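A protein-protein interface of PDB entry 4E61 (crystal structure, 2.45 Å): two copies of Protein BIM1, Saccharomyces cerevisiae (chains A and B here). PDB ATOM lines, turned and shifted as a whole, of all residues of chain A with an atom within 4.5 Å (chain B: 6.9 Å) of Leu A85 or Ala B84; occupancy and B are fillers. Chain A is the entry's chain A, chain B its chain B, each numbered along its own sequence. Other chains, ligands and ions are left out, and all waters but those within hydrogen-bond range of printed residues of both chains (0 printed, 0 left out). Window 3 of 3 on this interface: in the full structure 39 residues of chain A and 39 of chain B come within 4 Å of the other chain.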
ATOM      1  N   ILE A  62      21.270  18.218 -16.647  1.00  0.00           N
ATOM      2  CA  ILE A  62      20.911  17.006 -17.399  1.00  0.00           C
ATOM      3  C   ILE A  62      20.777  17.372 -18.892  1.00  0.00           C
ATOM      4  O   ILE A  62      21.283  16.637 -19.749  1.00  0.00           O
ATOM      5  CB  ILE A  62      19.655  16.265 -16.835  1.00  0.00           C
ATOM      6  CG1 ILE A  62      19.826  15.890 -15.338  1.00  0.00           C
ATOM      7  CG2 ILE A  62      19.333  15.010 -17.673  1.00  0.00           C
ATOM      8  CD1 ILE A  62      18.526  15.698 -14.563  1.00  0.00           C
ATOM      9  N   GLY A  83      18.485   9.203 -16.892  1.00  0.00           N
ATOM     10  CA  GLY A  83      17.964   7.886 -16.545  1.00  0.00           C
ATOM     11  C   GLY A  83      16.869   7.975 -15.507  1.00  0.00           C
ATOM     12  O   GLY A  83      15.863   8.655 -15.729  1.00  0.00           O
ATOM     13  N   ALA A  84      17.075   7.313 -14.357  1.00  0.00           N
ATOM     14  CA  ALA A  84      16.134   7.315 -13.226  1.00  0.00           C
ATOM     15  C   ALA A  84      16.074   8.694 -12.547  1.00  0.00           C
ATOM     16  O   ALA A  84      15.022   9.064 -12.017  1.00  0.00           O
ATOM     17  CB  ALA A  84      16.522   6.246 -12.213  1.00  0.00           C
ATOM     18  N   LEU A  85      17.194   9.445 -12.566  1.00  0.00           N
ATOM     19  CA  LEU A  85      17.282  10.782 -11.984  1.00  0.00           C
ATOM     20  C   LEU A  85      16.337  11.765 -12.699  1.00  0.00           C
ATOM     21  O   LEU A  85      15.598  12.486 -12.019  1.00  0.00           O
ATOM     22  CB  LEU A  85      18.736  11.299 -11.986  1.00  0.00           C
ATOM     23  CG  LEU A  85      18.968  12.770 -11.584  1.00  0.00           C
ATOM     24  CD1 LEU A  85      18.518  13.039 -10.160  1.00  0.00           C
ATOM     25  CD2 LEU A  85      20.413  13.174 -11.790  1.00  0.00           C
ATOM     26  N   LEU A  86      16.355  11.775 -14.059  1.00  0.00           N
ATOM     27  CA  LEU A  86      15.515  12.648 -14.888  1.00  0.00           C
ATOM     28  C   LEU A  86      14.024  12.334 -14.700  1.00  0.00           C
ATOM     29  O   LEU A  86      13.200  13.246 -14.665  1.00  0.00           O
ATOM     30  CB  LEU A  86      15.928  12.565 -16.367  1.00  0.00           C
ATOM     31  CG  LEU A  86      15.227  13.533 -17.328  1.00  0.00           C
ATOM     32  CD1 LEU A  86      15.654  15.004 -17.087  1.00  0.00           C
ATOM     33  CD2 LEU A  86      15.468  13.124 -18.760  1.00  0.00           C
ATOM     34  N   ARG A  87      13.708  11.053 -14.528  1.00  0.00           N
ATOM     35  CA  ARG A  87      12.363  10.533 -14.285  1.00  0.00           C
ATOM     36  C   ARG A  87      11.840  11.107 -12.965  1.00  0.00           C
ATOM     37  O   ARG A  87      10.708  11.590 -12.899  1.00  0.00           O
ATOM     38  CB  ARG A  87      12.423   8.997 -14.193  1.00  0.00           C
ATOM     39  CG  ARG A  87      11.216   8.255 -14.738  1.00  0.00           C
ATOM     40  CD  ARG A  87      11.490   6.760 -14.766  1.00  0.00           C
ATOM     41  NE  ARG A  87      12.562   6.416 -15.702  1.00  0.00           N
ATOM     42  CZ  ARG A  87      13.439   5.433 -15.512  1.00  0.00           C
ATOM     43  NH1 ARG A  87      13.369   4.670 -14.427  1.00  0.00           N
ATOM     44  NH2 ARG A  87      14.390   5.203 -16.408  1.00  0.00           N
ATOM     45  N   PHE A  88      12.687  11.078 -11.931  1.00  0.00           N
ATOM     46  CA  PHE A  88      12.361  11.595 -10.612  1.00  0.00           C
ATOM     47  C   PHE A  88      12.229  13.102 -10.667  1.00  0.00           C
ATOM     48  O   PHE A  88      11.236  13.623 -10.165  1.00  0.00           O
ATOM     49  CB  PHE A  88      13.408  11.159  -9.574  1.00  0.00           C
ATOM     50  CG  PHE A  88      13.085  11.587  -8.166  1.00  0.00           C
ATOM     51  CD1 PHE A  88      12.225  10.841  -7.378  1.00  0.00           C
ATOM     52  CD2 PHE A  88      13.607  12.764  -7.640  1.00  0.00           C
ATOM     53  CE1 PHE A  88      11.932  11.240  -6.071  1.00  0.00           C
ATOM     54  CE2 PHE A  88      13.288  13.175  -6.341  1.00  0.00           C
ATOM     55  CZ  PHE A  88      12.463  12.405  -5.564  1.00  0.00           C
ATOM     56  N   VAL A  89      13.194  13.793 -11.308  1.00  0.00           N
ATOM     57  CA  VAL A  89      13.193  15.251 -11.463  1.00  0.00           C
ATOM     58  C   VAL A  89      11.911  15.702 -12.159  1.00  0.00           C
ATOM     59  O   VAL A  89      11.301  16.671 -11.706  1.00  0.00           O
ATOM     60  CB  VAL A  89      14.494  15.805 -12.123  1.00  0.00           C
ATOM     61  CG1 VAL A  89      14.364  17.285 -12.460  1.00  0.00           C
ATOM     62  CG2 VAL A  89      15.699  15.600 -11.223  1.00  0.00           C
ATOM     63  N   GLY B  82      21.767   5.101  -4.586  1.00  0.00           N
ATOM     64  CA  GLY B  82      21.150   5.293  -5.898  1.00  0.00           C
ATOM     65  C   GLY B  82      21.947   6.158  -6.858  1.00  0.00           C
ATOM     66  O   GLY B  82      21.428   6.567  -7.905  1.00  0.00           O
ATOM     67  N   GLY B  83      23.214   6.404  -6.511  1.00  0.00           N
ATOM     68  CA  GLY B  83      24.121   7.240  -7.282  1.00  0.00           C
ATOM     69  C   GLY B  83      23.703   8.691  -7.209  1.00  0.00           C
ATOM     70  O   GLY B  83      23.533   9.243  -6.116  1.00  0.00           O
ATOM     71  N   ALA B  84      23.503   9.304  -8.383  1.00  0.00           N
ATOM     72  CA  ALA B  84      23.071  10.700  -8.519  1.00  0.00           C
ATOM     73  C   ALA B  84      21.611  10.881  -8.053  1.00  0.00           C
ATOM     74  O   ALA B  84      21.261  11.952  -7.566  1.00  0.00           O
ATOM     75  CB  ALA B  84      23.225  11.158  -9.965  1.00  0.00           C
ATOM     76  N   LEU B  85      20.778   9.831  -8.209  1.00  0.00           N
ATOM     77  CA  LEU B  85      19.382   9.827  -7.803  1.00  0.00           C
ATOM     78  C   LEU B  85      19.242  10.009  -6.293  1.00  0.00           C
ATOM     79  O   LEU B  85      18.465  10.870  -5.871  1.00  0.00           O
ATOM     80  CB  LEU B  85      18.651   8.554  -8.284  1.00  0.00           C
ATOM     81  CG  LEU B  85      17.185   8.372  -7.833  1.00  0.00           C
ATOM     82  CD1 LEU B  85      16.297   9.507  -8.304  1.00  0.00           C
ATOM     83  CD2 LEU B  85      16.631   7.031  -8.274  1.00  0.00           C
ATOM     84  N   LEU B  86      20.009   9.222  -5.494  1.00  0.00           N
ATOM     85  CA  LEU B  86      20.023   9.281  -4.027  1.00  0.00           C
ATOM     86  C   LEU B  86      20.490  10.645  -3.514  1.00  0.00           C
ATOM     87  O   LEU B  86      19.932  11.164  -2.544  1.00  0.00           O
ATOM     88  CB  LEU B  86      20.866   8.142  -3.429  1.00  0.00           C
ATOM     89  CG  LEU B  86      20.869   8.008  -1.904  1.00  0.00           C
ATOM     90  CD1 LEU B  86      19.555   7.503  -1.400  1.00  0.00           C
ATOM     91  CD2 LEU B  86      21.982   7.100  -1.443  1.00  0.00           C
ATOM     92  N   ARG B  87      21.476  11.231  -4.196  1.00  0.00           N
ATOM     93  CA  ARG B  87      22.040  12.548  -3.903  1.00  0.00           C
ATOM     94  C   ARG B  87      20.952  13.610  -4.057  1.00  0.00           C
ATOM     95  O   ARG B  87      20.793  14.467  -3.181  1.00  0.00           O
ATOM     96  CB  ARG B  87      23.175  12.823  -4.894  1.00  0.00           C
ATOM     97  CG  ARG B  87      24.347  13.612  -4.333  1.00  0.00           C
ATOM     98  CD  ARG B  87      25.487  13.649  -5.342  1.00  0.00           C
ATOM     99  NE  ARG B  87      26.031  12.314  -5.606  1.00  0.00           N
ATOM    100  CZ  ARG B  87      26.482  11.902  -6.787  1.00  0.00           C
ATOM    101  NH1 ARG B  87      26.469  12.721  -7.835  1.00  0.00           N
ATOM    102  NH2 ARG B  87      26.947  10.670  -6.930  1.00  0.00           N
ATOM    103  N   PHE B  88      20.181  13.519  -5.156  1.00  0.00           N
ATOM    104  CA  PHE B  88      19.093  14.435  -5.448  1.00  0.00           C
ATOM    105  C   PHE B  88      17.962  14.229  -4.452  1.00  0.00           C
ATOM    106  O   PHE B  88      17.480  15.205  -3.882  1.00  0.00           O
ATOM    107  CB  PHE B  88      18.607  14.283  -6.891  1.00  0.00           C
ATOM    108  CG  PHE B  88      17.547  15.294  -7.272  1.00  0.00           C
ATOM    109  CD1 PHE B  88      17.897  16.581  -7.668  1.00  0.00           C
ATOM    110  CD2 PHE B  88      16.198  14.969  -7.209  1.00  0.00           C
ATOM    111  CE1 PHE B  88      16.907  17.536  -7.969  1.00  0.00           C
ATOM    112  CE2 PHE B  88      15.212  15.921  -7.522  1.00  0.00           C
ATOM    113  CZ  PHE B  88      15.575  17.196  -7.900  1.00  0.00           C
ATOM    114  N   VAL B  89      17.566  12.968  -4.219  1.00  0.00           N
ATOM    115  CA  VAL B  89      16.526  12.605  -3.257  1.00  0.00           C
ATOM    116  C   VAL B  89      16.863  13.154  -1.863  1.00  0.00           C
ATOM    117  O   VAL B  89      15.982  13.707  -1.211  1.00  0.00           O
ATOM    118  CB  VAL B  89      16.201  11.090  -3.277  1.00  0.00           C
ATOM    119  CG1 VAL B  89      15.309  10.694  -2.104  1.00  0.00           C
ATOM    120  CG2 VAL B  89      15.536  10.698  -4.597  1.00  0.00           C
ATOM    121  N   LYS B  91      18.854  15.797  -1.223  1.00  0.00           N
ATOM    122  CA  LYS B  91      18.813  17.251  -1.334  1.00  0.00           C
ATOM    123  C   LYS B  91      17.368  17.744  -1.114  1.00  0.00           C
ATOM    124  O   LYS B  91      17.170  18.694  -0.361  1.00  0.00           O
ATOM    125  CB  LYS B  91      19.349  17.703  -2.697  1.00  0.00           C
ATOM    126  CG  LYS B  91      20.866  17.838  -2.747  1.00  0.00           C
ATOM    127  CD  LYS B  91      21.391  18.245  -4.135  1.00  0.00           C
ATOM    128  CE  LYS B  91      22.219  17.145  -4.764  1.00  0.00           C
ATOM    129  NZ  LYS B  91      22.639  17.479  -6.148  1.00  0.00           N
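Hydrophobic or aromatic side chains of chain A that line the printed part of chain B: Leu A85, Phe A88 and Val A89.
Hydrophobic or aromatic side chains of chain B that line the printed part of chain A: Ala B84, Leu B85, Phe B88 and Val B89.
Along chain B the printed residues that touch a printed residue of chain A span positions 84 to 89.
Among the printed residues, no Asp or Glu carboxylate lies within 4 Å of a Lys or Arg side-chain nitrogen of the other chain.
Among the printed residues, merely in contact across the chains: Phe A88 with Phe B88, Leu A85 with Phe B88, Phe A88 with Leu B85, Phe A88 with Val B89, Val A89 with Phe B88, Leu A85 with Ala B84 and Ala A84 with Leu B85.
Ala A84 touches Leu B85, and with the chains exchanged Leu A85 touches Ala B84.
Leu A85 touches Phe B88, and with the chains exchanged Phe A88 touches Leu B85.
Phe B88 touches its own counterpart, Phe A88.
Phe A88 touches Val B89, and with the chains exchanged Val A89 touches Phe B88.
Positions printed for both chains: 83, 84, 85, 86, 87, 88 and 89.
Of the 7 pairs that touch across the chains among the printed residues, 7 have their exchanged pair printed and touching as well.
Printed residues of chain B within 4 Å of Leu A85: Ala B84 and Phe B88.
Of the printed residues of chain B, Phe A88 touches Leu B85, Phe B88 and Val B89.
Of the printed residues of chain B, Val A89 touches Phe B88 (3.7 Å).
Gly B82 touches none of the printed residues of chain A.
Of chain A, only Leu A85 (3.9 Å) comes within 4 Å of Ala B84.
Printed residues of chain A within 4 Å of Val B89: Phe A88 (3.6 Å).
Lys B91 touches none of the printed residues of chain A.
The nearest printed residue of chain B that does not touch Leu A85 is Leu B85 (4.02 Å).
The nearest printed residue of chain A that does not touch Leu B85 is Leu A85 (4.02 Å).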
